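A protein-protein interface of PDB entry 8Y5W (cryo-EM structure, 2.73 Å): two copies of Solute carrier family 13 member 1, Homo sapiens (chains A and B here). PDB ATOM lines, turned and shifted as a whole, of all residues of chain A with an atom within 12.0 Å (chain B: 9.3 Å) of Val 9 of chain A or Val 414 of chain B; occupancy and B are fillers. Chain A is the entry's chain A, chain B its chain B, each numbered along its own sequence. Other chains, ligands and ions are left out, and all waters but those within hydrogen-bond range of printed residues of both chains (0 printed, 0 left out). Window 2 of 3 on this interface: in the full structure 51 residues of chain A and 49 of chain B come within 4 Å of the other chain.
The side-chain hydroxyl (OH) of Tyr 418 of chain B sits at hydrogen-bond distance from the backbone NH (N) of Phe 13 of chain A.
The side-chain carboxylate (OD2) of Asp 417 of chain B is in salt-bridge range of the guanidinium group (NH1) of Arg 12 of chain A, 2.8 Å away.
The guanidinium group (NH1) of Arg 11 of chain A lies within hydrogen-bond range of the backbone carbonyl oxygen (O) of Phe 416 of chain B (3.2 Å).
The guanidinium group (NH2) of Arg 12 of chain A lies within hydrogen-bond range of the backbone carbonyl oxygen (O) of Tyr 418 of chain B, 2.8 Å away.
N of Leu 404 of chain B sits at hydrogen-bond distance from O of Asp 417 of chain B, at 2.7 Å.
The backbone carbonyl oxygen of Leu 8 of chain A lies within hydrogen-bond range of the guanidinium group of Arg 11 of chain A, 2.6 Å away.
Among the printed residues, pairs that only touch across the chains: Val 9 of chain A with Asp 417 of chain B (3.4 Å), Tyr 10 of chain A with Tyr 418 of chain B (3.5 Å), Val 9 of chain A with Tyr 418 of chain B (3.5 Å), Val 9 of chain A with Val 414 of chain B (3.6 Å), Leu 8 of chain A with Phe 416 of chain B (3.7 Å), Arg 11 of chain A with Asp 417 of chain B (3.8 Å) and Val 9 of chain A with Phe 416 of chain B (3.9 Å).
Printed residues of chain B within 4 Å of Leu 8 of chain A: Phe 416.
Printed residues of chain B within 4 Å of Val 9 of chain A: Val 414, Phe 416, Asp 417 and Tyr 418.
Of chain B, only Tyr 418 comes within 4 Å of Tyr 10 of chain A.
Of the printed residues of chain B, Arg 12 of chain A touches Asp 417 (2.8 Å) and Tyr 418 (2.8 Å).
No residue of chain A comes within 4 Å of Ile 413 of chain B.
Of chain A, only Val 9 (3.6 Å) comes within 4 Å of Val 414 of chain B.
No residue of chain A comes within 4 Å of Ala 415 of chain B.
Of the printed residues of chain A, Phe 416 of chain B touches Leu 8 (3.7 Å), Val 9 (3.9 Å) and Arg 11 (3.2 Å).
Of the printed residues of chain A, Asp 417 of chain B touches Val 9, Arg 11 and Arg 12.
The nearest printed residue of chain A that does not touch Phe 416 of chain B is Tyr 10 of chain A (5.9 Å).
Of the 17 printed residues of chain A, 6 touch a printed residue of chain B.
Hydrophobic or aromatic side chains of chain A that line the printed part of chain B: Val 9, Tyr 10 and Phe 13.
Along chain A the printed residues that touch a printed residue of chain B span positions 8 to 13.
Of the 12 printed residues of chain B, 4 touch a printed residue of chain A.
Among the printed residues, 11 pairs touch across the chains.
Among the printed residues, Asp or Glu carboxylates within 4 Å of a Lys or Arg side-chain nitrogen of the other chain: Arg 12 of chain A with Asp 417 of chain B (2.8 Å).
No position is printed for both chains.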
ATOM      1  N   LYS A   2     -13.846   2.991   2.177  1.00  0.00           N
ATOM      2  CA  LYS A   2     -12.425   3.311   2.250  1.00  0.00           C
ATOM      3  C   LYS A   2     -11.697   2.361   3.198  1.00  0.00           C
ATOM      4  O   LYS A   2     -10.507   2.094   3.030  1.00  0.00           O
ATOM      5  CB  LYS A   2     -12.226   4.763   2.695  1.00  0.00           C
ATOM      6  CG  LYS A   2     -12.788   5.080   4.071  1.00  0.00           C
ATOM      7  CD  LYS A   2     -12.642   6.554   4.406  1.00  0.00           C
ATOM      8  CE  LYS A   2     -13.188   6.860   5.790  1.00  0.00           C
ATOM      9  NZ  LYS A   2     -14.661   6.664   5.863  1.00  0.00           N
ATOM     10  N   PHE A   3     -12.416   1.856   4.190  1.00  0.00           N
ATOM     11  CA  PHE A   3     -11.864   0.916   5.159  1.00  0.00           C
ATOM     12  C   PHE A   3     -12.684  -0.359   5.277  1.00  0.00           C
ATOM     13  O   PHE A   3     -12.111  -1.433   5.473  1.00  0.00           O
ATOM     14  CB  PHE A   3     -11.749   1.586   6.536  1.00  0.00           C
ATOM     15  CG  PHE A   3     -11.105   0.720   7.581  1.00  0.00           C
ATOM     16  CD1 PHE A   3      -9.738   0.505   7.573  1.00  0.00           C
ATOM     17  CD2 PHE A   3     -11.868   0.121   8.570  1.00  0.00           C
ATOM     18  CE1 PHE A   3      -9.141  -0.291   8.532  1.00  0.00           C
ATOM     19  CE2 PHE A   3     -11.277  -0.676   9.531  1.00  0.00           C
ATOM     20  CZ  PHE A   3      -9.912  -0.882   9.512  1.00  0.00           C
ATOM     21  N   PHE A   4     -14.011  -0.268   5.165  1.00  0.00           N
ATOM     22  CA  PHE A   4     -14.849  -1.458   5.229  1.00  0.00           C
ATOM     23  C   PHE A   4     -14.731  -2.305   3.969  1.00  0.00           C
ATOM     24  O   PHE A   4     -14.925  -3.523   4.037  1.00  0.00           O
ATOM     25  CB  PHE A   4     -16.306  -1.051   5.470  1.00  0.00           C
ATOM     26  CG  PHE A   4     -17.194  -2.182   5.914  1.00  0.00           C
ATOM     27  CD1 PHE A   4     -17.752  -3.055   4.993  1.00  0.00           C
ATOM     28  CD2 PHE A   4     -17.470  -2.372   7.258  1.00  0.00           C
ATOM     29  CE1 PHE A   4     -18.566  -4.092   5.404  1.00  0.00           C
ATOM     30  CE2 PHE A   4     -18.284  -3.407   7.675  1.00  0.00           C
ATOM     31  CZ  PHE A   4     -18.832  -4.269   6.747  1.00  0.00           C
ATOM     32  N   SER A   5     -14.408  -1.690   2.829  1.00  0.00           N
ATOM     33  CA  SER A   5     -14.271  -2.447   1.588  1.00  0.00           C
ATOM     34  C   SER A   5     -13.142  -3.465   1.668  1.00  0.00           C
ATOM     35  O   SER A   5     -13.285  -4.585   1.166  1.00  0.00           O
ATOM     36  CB  SER A   5     -14.045  -1.494   0.415  1.00  0.00           C
ATOM     37  OG  SER A   5     -12.812  -0.807   0.544  1.00  0.00           O
ATOM     38  N   TYR A   6     -12.019  -3.102   2.290  1.00  0.00           N
ATOM     39  CA  TYR A   6     -10.900  -4.024   2.438  1.00  0.00           C
ATOM     40  C   TYR A   6     -11.214  -5.197   3.357  1.00  0.00           C
ATOM     41  O   TYR A   6     -10.566  -6.242   3.240  1.00  0.00           O
ATOM     42  CB  TYR A   6      -9.669  -3.283   2.967  1.00  0.00           C
ATOM     43  CG  TYR A   6      -9.087  -2.274   2.002  1.00  0.00           C
ATOM     44  CD1 TYR A   6      -9.447  -2.275   0.660  1.00  0.00           C
ATOM     45  CD2 TYR A   6      -8.174  -1.321   2.434  1.00  0.00           C
ATOM     46  CE1 TYR A   6      -8.916  -1.354  -0.222  1.00  0.00           C
ATOM     47  CE2 TYR A   6      -7.637  -0.397   1.559  1.00  0.00           C
ATOM     48  CZ  TYR A   6      -8.011  -0.418   0.232  1.00  0.00           C
ATOM     49  OH  TYR A   6      -7.479   0.502  -0.642  1.00  0.00           O
ATOM     50  N   ILE A   7     -12.180  -5.052   4.262  1.00  0.00           N
ATOM     51  CA  ILE A   7     -12.521  -6.139   5.175  1.00  0.00           C
ATOM     52  C   ILE A   7     -13.198  -7.279   4.426  1.00  0.00           C
ATOM     53  O   ILE A   7     -12.882  -8.455   4.639  1.00  0.00           O
ATOM     54  CB  ILE A   7     -13.403  -5.613   6.322  1.00  0.00           C
ATOM     55  CG1 ILE A   7     -12.666  -4.525   7.104  1.00  0.00           C
ATOM     56  CG2 ILE A   7     -13.805  -6.748   7.248  1.00  0.00           C
ATOM     57  CD1 ILE A   7     -11.396  -5.005   7.766  1.00  0.00           C
ATOM     58  N   LEU A   8     -14.135  -6.954   3.538  1.00  0.00           N
ATOM     59  CA  LEU A   8     -14.872  -7.968   2.793  1.00  0.00           C
ATOM     60  C   LEU A   8     -14.060  -8.588   1.665  1.00  0.00           C
ATOM     61  O   LEU A   8     -14.507  -9.578   1.074  1.00  0.00           O
ATOM     62  CB  LEU A   8     -16.176  -7.370   2.249  1.00  0.00           C
ATOM     63  CG  LEU A   8     -16.147  -6.194   1.265  1.00  0.00           C
ATOM     64  CD1 LEU A   8     -15.936  -6.636  -0.182  1.00  0.00           C
ATOM     65  CD2 LEU A   8     -17.420  -5.369   1.392  1.00  0.00           C
ATOM     66  N   VAL A   9     -12.893  -8.036   1.344  1.00  0.00           N
ATOM     67  CA  VAL A   9     -12.026  -8.634   0.335  1.00  0.00           C
ATOM     68  C   VAL A   9     -11.104  -9.677   0.952  1.00  0.00           C
ATOM     69  O   VAL A   9     -10.948 -10.775   0.414  1.00  0.00           O
ATOM     70  CB  VAL A   9     -11.228  -7.534  -0.390  1.00  0.00           C
ATOM     71  CG1 VAL A   9     -10.225  -8.149  -1.351  1.00  0.00           C
ATOM     72  CG2 VAL A   9     -12.169  -6.597  -1.121  1.00  0.00           C
ATOM     73  N   TYR A  10     -10.492  -9.352   2.085  1.00  0.00           N
ATOM     74  CA  TYR A  10      -9.615 -10.282   2.797  1.00  0.00           C
ATOM     75  C   TYR A  10     -10.401 -11.028   3.874  1.00  0.00           C
ATOM     76  O   TYR A  10     -10.065 -11.016   5.056  1.00  0.00           O
ATOM     77  CB  TYR A  10      -8.430  -9.528   3.391  1.00  0.00           C
ATOM     78  CG  TYR A  10      -7.611  -8.785   2.361  1.00  0.00           C
ATOM     79  CD1 TYR A  10      -7.443  -9.292   1.081  1.00  0.00           C
ATOM     80  CD2 TYR A  10      -7.021  -7.566   2.664  1.00  0.00           C
ATOM     81  CE1 TYR A  10      -6.702  -8.615   0.135  1.00  0.00           C
ATOM     82  CE2 TYR A  10      -6.278  -6.879   1.722  1.00  0.00           C
ATOM     83  CZ  TYR A  10      -6.123  -7.410   0.460  1.00  0.00           C
ATOM     84  OH  TYR A  10      -5.384  -6.732  -0.483  1.00  0.00           O
ATOM     85  N   ARG A  11     -11.475 -11.686   3.436  1.00  0.00           N
ATOM     86  CA  ARG A  11     -12.341 -12.396   4.372  1.00  0.00           C
ATOM     87  C   ARG A  11     -11.643 -13.613   4.964  1.00  0.00           C
ATOM     88  O   ARG A  11     -11.680 -13.828   6.180  1.00  0.00           O
ATOM     89  CB  ARG A  11     -13.639 -12.806   3.677  1.00  0.00           C
ATOM     90  CG  ARG A  11     -14.621 -11.669   3.476  1.00  0.00           C
ATOM     91  CD  ARG A  11     -15.899 -12.145   2.799  1.00  0.00           C
ATOM     92  NE  ARG A  11     -15.671 -13.283   1.918  1.00  0.00           N
ATOM     93  CZ  ARG A  11     -15.176 -13.195   0.692  1.00  0.00           C
ATOM     94  NH1 ARG A  11     -14.843 -12.028   0.164  1.00  0.00           N
ATOM     95  NH2 ARG A  11     -15.009 -14.302  -0.024  1.00  0.00           N
ATOM     96  N   ARG A  12     -11.009 -14.429   4.119  1.00  0.00           N
ATOM     97  CA  ARG A  12     -10.385 -15.654   4.610  1.00  0.00           C
ATOM     98  C   ARG A  12      -9.210 -15.367   5.536  1.00  0.00           C
ATOM     99  O   ARG A  12      -9.092 -16.000   6.589  1.00  0.00           O
ATOM    100  CB  ARG A  12      -9.931 -16.523   3.438  1.00  0.00           C
ATOM    101  CG  ARG A  12     -11.069 -17.157   2.660  1.00  0.00           C
ATOM    102  CD  ARG A  12     -10.546 -18.076   1.570  1.00  0.00           C
ATOM    103  NE  ARG A  12      -9.656 -17.378   0.649  1.00  0.00           N
ATOM    104  CZ  ARG A  12     -10.065 -16.617  -0.358  1.00  0.00           C
ATOM    105  NH1 ARG A  12     -11.350 -16.420  -0.599  1.00  0.00           N
ATOM    106  NH2 ARG A  12      -9.160 -16.038  -1.141  1.00  0.00           N
ATOM    107  N   PHE A  13      -8.338 -14.425   5.168  1.00  0.00           N
ATOM    108  CA  PHE A  13      -7.175 -14.124   5.997  1.00  0.00           C
ATOM    109  C   PHE A  13      -7.595 -13.596   7.364  1.00  0.00           C
ATOM    110  O   PHE A  13      -7.134 -14.088   8.405  1.00  0.00           O
ATOM    111  CB  PHE A  13      -6.277 -13.114   5.282  1.00  0.00           C
ATOM    112  CG  PHE A  13      -5.016 -12.785   6.028  1.00  0.00           C
ATOM    113  CD1 PHE A  13      -3.924 -13.632   5.976  1.00  0.00           C
ATOM    114  CD2 PHE A  13      -4.923 -11.628   6.781  1.00  0.00           C
ATOM    115  CE1 PHE A  13      -2.763 -13.330   6.660  1.00  0.00           C
ATOM    116  CE2 PHE A  13      -3.767 -11.322   7.469  1.00  0.00           C
ATOM    117  CZ  PHE A  13      -2.686 -12.174   7.407  1.00  0.00           C
ATOM    118  N   LEU A  14      -8.472 -12.592   7.379  1.00  0.00           N
ATOM    119  CA  LEU A  14      -8.963 -12.028   8.625  1.00  0.00           C
ATOM    120  C   LEU A  14      -9.743 -13.031   9.457  1.00  0.00           C
ATOM    121  O   LEU A  14      -9.593 -13.036  10.679  1.00  0.00           O
ATOM    122  CB  LEU A  14      -9.831 -10.799   8.346  1.00  0.00           C
ATOM    123  CG  LEU A  14      -9.092  -9.590   7.771  1.00  0.00           C
ATOM    124  CD1 LEU A  14     -10.062  -8.464   7.460  1.00  0.00           C
ATOM    125  CD2 LEU A  14      -8.007  -9.121   8.727  1.00  0.00           C
ATOM    126  N   PHE A  15     -10.560 -13.880   8.833  1.00  0.00           N
ATOM    127  CA  PHE A  15     -11.255 -14.929   9.564  1.00  0.00           C
ATOM    128  C   PHE A  15     -10.306 -15.945  10.178  1.00  0.00           C
ATOM    129  O   PHE A  15     -10.529 -16.372  11.313  1.00  0.00           O
ATOM    130  CB  PHE A  15     -12.247 -15.654   8.653  1.00  0.00           C
ATOM    131  CG  PHE A  15     -13.000 -16.758   9.341  1.00  0.00           C
ATOM    132  CD1 PHE A  15     -13.998 -16.466  10.256  1.00  0.00           C
ATOM    133  CD2 PHE A  15     -12.703 -18.084   9.083  1.00  0.00           C
ATOM    134  CE1 PHE A  15     -14.689 -17.478  10.894  1.00  0.00           C
ATOM    135  CE2 PHE A  15     -13.390 -19.099   9.719  1.00  0.00           C
ATOM    136  CZ  PHE A  15     -14.384 -18.795  10.625  1.00  0.00           C
ATOM    137  N   VAL A  16      -9.255 -16.348   9.459  1.00  0.00           N
ATOM    138  CA  VAL A  16      -8.288 -17.282  10.026  1.00  0.00           C
ATOM    139  C   VAL A  16      -7.572 -16.653  11.215  1.00  0.00           C
ATOM    140  O   VAL A  16      -7.412 -17.286  12.267  1.00  0.00           O
ATOM    141  CB  VAL A  16      -7.297 -17.746   8.943  1.00  0.00           C
ATOM    142  CG1 VAL A  16      -6.100 -18.437   9.575  1.00  0.00           C
ATOM    143  CG2 VAL A  16      -7.987 -18.673   7.959  1.00  0.00           C
ATOM    144  N   GLU A  51     -14.215 -23.873   5.539  1.00  0.00           N
ATOM    145  CA  GLU A  51     -13.244 -24.011   4.456  1.00  0.00           C
ATOM    146  C   GLU A  51     -12.517 -22.684   4.213  1.00  0.00           C
ATOM    147  O   GLU A  51     -12.399 -22.191   3.091  1.00  0.00           O
ATOM    148  CB  GLU A  51     -13.920 -24.533   3.185  1.00  0.00           C
ATOM    149  CG  GLU A  51     -12.964 -24.974   2.083  1.00  0.00           C
ATOM    150  CD  GLU A  51     -13.491 -26.154   1.290  1.00  0.00           C
ATOM    151  OE1 GLU A  51     -12.796 -26.602   0.354  1.00  0.00           O
ATOM    152  OE2 GLU A  51     -14.600 -26.635   1.603  1.00  0.00           O
ATOM    153  N   ALA A  52     -12.042 -22.095   5.314  1.00  0.00           N
ATOM    154  CA  ALA A  52     -11.217 -20.897   5.216  1.00  0.00           C
ATOM    155  C   ALA A  52      -9.840 -21.213   4.655  1.00  0.00           C
ATOM    156  O   ALA A  52      -9.250 -20.383   3.956  1.00  0.00           O
ATOM    157  CB  ALA A  52     -11.091 -20.228   6.584  1.00  0.00           C
ATOM    158  N   PRO B 400      -1.820 -13.222   1.305  1.00  0.00           N
ATOM    159  CA  PRO B 400      -2.286 -12.800  -0.020  1.00  0.00           C
ATOM    160  C   PRO B 400      -1.137 -12.531  -0.979  1.00  0.00           C
ATOM    161  O   PRO B 400      -0.065 -12.060  -0.593  1.00  0.00           O
ATOM    162  CB  PRO B 400      -3.068 -11.514   0.273  1.00  0.00           C
ATOM    163  CG  PRO B 400      -3.426 -11.607   1.720  1.00  0.00           C
ATOM    164  CD  PRO B 400      -2.277 -12.310   2.366  1.00  0.00           C
ATOM    165  N   LYS B 402      -2.196 -11.866  -4.871  1.00  0.00           N
ATOM    166  CA  LYS B 402      -2.867 -11.005  -5.832  1.00  0.00           C
ATOM    167  C   LYS B 402      -4.287 -10.721  -5.361  1.00  0.00           C
ATOM    168  O   LYS B 402      -4.796 -11.344  -4.425  1.00  0.00           O
ATOM    169  CB  LYS B 402      -2.888 -11.640  -7.228  1.00  0.00           C
ATOM    170  CG  LYS B 402      -1.542 -11.654  -7.931  1.00  0.00           C
ATOM    171  CD  LYS B 402      -1.673 -12.187  -9.348  1.00  0.00           C
ATOM    172  CE  LYS B 402      -0.326 -12.243 -10.048  1.00  0.00           C
ATOM    173  NZ  LYS B 402       0.220 -10.884 -10.314  1.00  0.00           N
ATOM    174  N   THR B 403      -4.925  -9.766  -6.026  1.00  0.00           N
ATOM    175  CA  THR B 403      -6.294  -9.367  -5.724  1.00  0.00           C
ATOM    176  C   THR B 403      -7.183  -9.749  -6.899  1.00  0.00           C
ATOM    177  O   THR B 403      -6.912  -9.360  -8.040  1.00  0.00           O
ATOM    178  CB  THR B 403      -6.378  -7.867  -5.451  1.00  0.00           C
ATOM    179  OG1 THR B 403      -5.412  -7.506  -4.456  1.00  0.00           O
ATOM    180  CG2 THR B 403      -7.758  -7.502  -4.949  1.00  0.00           C
ATOM    181  N   LEU B 404      -8.239 -10.507  -6.621  1.00  0.00           N
ATOM    182  CA  LEU B 404      -9.159 -10.941  -7.666  1.00  0.00           C
ATOM    183  C   LEU B 404     -10.294  -9.939  -7.843  1.00  0.00           C
ATOM    184  O   LEU B 404     -10.076  -8.809  -8.282  1.00  0.00           O
ATOM    185  CB  LEU B 404      -9.724 -12.326  -7.345  1.00  0.00           C
ATOM    186  CG  LEU B 404      -8.722 -13.478  -7.279  1.00  0.00           C
ATOM    187  CD1 LEU B 404      -9.417 -14.773  -6.894  1.00  0.00           C
ATOM    188  CD2 LEU B 404      -7.991 -13.633  -8.602  1.00  0.00           C
ATOM    189  N   GLU B 412     -14.709  -0.905  -6.695  1.00  0.00           N
ATOM    190  CA  GLU B 412     -15.116  -1.224  -8.058  1.00  0.00           C
ATOM    191  C   GLU B 412     -14.016  -1.999  -8.776  1.00  0.00           C
ATOM    192  O   GLU B 412     -14.295  -2.902  -9.566  1.00  0.00           O
ATOM    193  CB  GLU B 412     -15.459   0.054  -8.829  1.00  0.00           C
ATOM    194  CG  GLU B 412     -16.315  -0.169 -10.069  1.00  0.00           C
ATOM    195  CD  GLU B 412     -15.488  -0.349 -11.327  1.00  0.00           C
ATOM    196  OE1 GLU B 412     -14.369   0.200 -11.391  1.00  0.00           O
ATOM    197  OE2 GLU B 412     -15.961  -1.038 -12.257  1.00  0.00           O
ATOM    198  N   ILE B 413     -12.765  -1.635  -8.498  1.00  0.00           N
ATOM    199  CA  ILE B 413     -11.631  -2.315  -9.117  1.00  0.00           C
ATOM    200  C   ILE B 413     -11.513  -3.745  -8.605  1.00  0.00           C
ATOM    201  O   ILE B 413     -11.361  -4.689  -9.389  1.00  0.00           O
ATOM    202  CB  ILE B 413     -10.335  -1.518  -8.877  1.00  0.00           C
ATOM    203  CG1 ILE B 413     -10.411  -0.152  -9.564  1.00  0.00           C
ATOM    204  CG2 ILE B 413      -9.127  -2.299  -9.370  1.00  0.00           C
ATOM    205  CD1 ILE B 413     -10.770   0.987  -8.633  1.00  0.00           C
ATOM    206  N   VAL B 414     -11.586  -3.929  -7.290  1.00  0.00           N
ATOM    207  CA  VAL B 414     -11.552  -5.263  -6.701  1.00  0.00           C
ATOM    208  C   VAL B 414     -12.895  -5.943  -6.925  1.00  0.00           C
ATOM    209  O   VAL B 414     -13.957  -5.349  -6.702  1.00  0.00           O
ATOM    210  CB  VAL B 414     -11.191  -5.189  -5.207  1.00  0.00           C
ATOM    211  CG1 VAL B 414     -12.165  -4.296  -4.453  1.00  0.00           C
ATOM    212  CG2 VAL B 414     -11.186  -6.581  -4.605  1.00  0.00           C
ATOM    213  N   ALA B 415     -12.858  -7.190  -7.401  1.00  0.00           N
ATOM    214  CA  ALA B 415     -14.111  -7.871  -7.724  1.00  0.00           C
ATOM    215  C   ALA B 415     -14.743  -8.513  -6.491  1.00  0.00           C
ATOM    216  O   ALA B 415     -15.793  -8.064  -6.018  1.00  0.00           O
ATOM    217  CB  ALA B 415     -13.868  -8.915  -8.819  1.00  0.00           C
ATOM    218  N   PHE B 416     -14.123  -9.563  -5.950  1.00  0.00           N
ATOM    219  CA  PHE B 416     -14.721 -10.201  -4.782  1.00  0.00           C
ATOM    220  C   PHE B 416     -13.749 -10.547  -3.652  1.00  0.00           C
ATOM    221  O   PHE B 416     -14.105 -10.389  -2.480  1.00  0.00           O
ATOM    222  CB  PHE B 416     -15.531 -11.430  -5.224  1.00  0.00           C
ATOM    223  CG  PHE B 416     -14.776 -12.407  -6.085  1.00  0.00           C
ATOM    224  CD1 PHE B 416     -14.603 -12.167  -7.439  1.00  0.00           C
ATOM    225  CD2 PHE B 416     -14.320 -13.602  -5.563  1.00  0.00           C
ATOM    226  CE1 PHE B 416     -13.931 -13.069  -8.239  1.00  0.00           C
ATOM    227  CE2 PHE B 416     -13.652 -14.514  -6.362  1.00  0.00           C
ATOM    228  CZ  PHE B 416     -13.456 -14.245  -7.700  1.00  0.00           C
ATOM    229  N   ASP B 417     -12.538 -11.002  -3.957  1.00  0.00           N
ATOM    230  CA  ASP B 417     -11.615 -11.374  -2.881  1.00  0.00           C
ATOM    231  C   ASP B 417     -10.188 -11.370  -3.425  1.00  0.00           C
ATOM    232  O   ASP B 417      -9.912 -10.803  -4.487  1.00  0.00           O
ATOM    233  CB  ASP B 417     -12.000 -12.733  -2.266  1.00  0.00           C
ATOM    234  CG  ASP B 417     -11.901 -13.879  -3.254  1.00  0.00           C
ATOM    235  OD1 ASP B 417     -11.570 -13.638  -4.431  1.00  0.00           O
ATOM    236  OD2 ASP B 417     -12.159 -15.032  -2.848  1.00  0.00           O
ATOM    237  N   TYR B 418      -9.279 -11.999  -2.684  1.00  0.00           N
ATOM    238  CA  TYR B 418      -7.870 -12.136  -3.022  1.00  0.00           C
ATOM    239  C   TYR B 418      -7.553 -13.595  -3.348  1.00  0.00           C
ATOM    240  O   TYR B 418      -8.428 -14.463  -3.343  1.00  0.00           O
ATOM    241  CB  TYR B 418      -6.990 -11.640  -1.871  1.00  0.00           C
ATOM    242  CG  TYR B 418      -6.924 -12.599  -0.701  1.00  0.00           C
ATOM    243  CD1 TYR B 418      -7.946 -12.656   0.235  1.00  0.00           C
ATOM    244  CD2 TYR B 418      -5.838 -13.448  -0.533  1.00  0.00           C
ATOM    245  CE1 TYR B 418      -7.889 -13.530   1.302  1.00  0.00           C
ATOM    246  CE2 TYR B 418      -5.772 -14.324   0.528  1.00  0.00           C
ATOM    247  CZ  TYR B 418      -6.800 -14.361   1.443  1.00  0.00           C
ATOM    248  OH  TYR B 418      -6.733 -15.235   2.503  1.00  0.00           O
ATOM    249  N   SER B 419      -6.276 -13.856  -3.629  1.00  0.00           N
ATOM    250  CA  SER B 419      -5.751 -15.199  -3.839  1.00  0.00           C
ATOM    251  C   SER B 419      -4.477 -15.349  -3.016  1.00  0.00           C
ATOM    252  O   SER B 419      -3.770 -14.357  -2.793  1.00  0.00           O
ATOM    253  CB  SER B 419      -5.456 -15.470  -5.321  1.00  0.00           C
ATOM    254  OG  SER B 419      -4.452 -14.598  -5.807  1.00  0.00           O
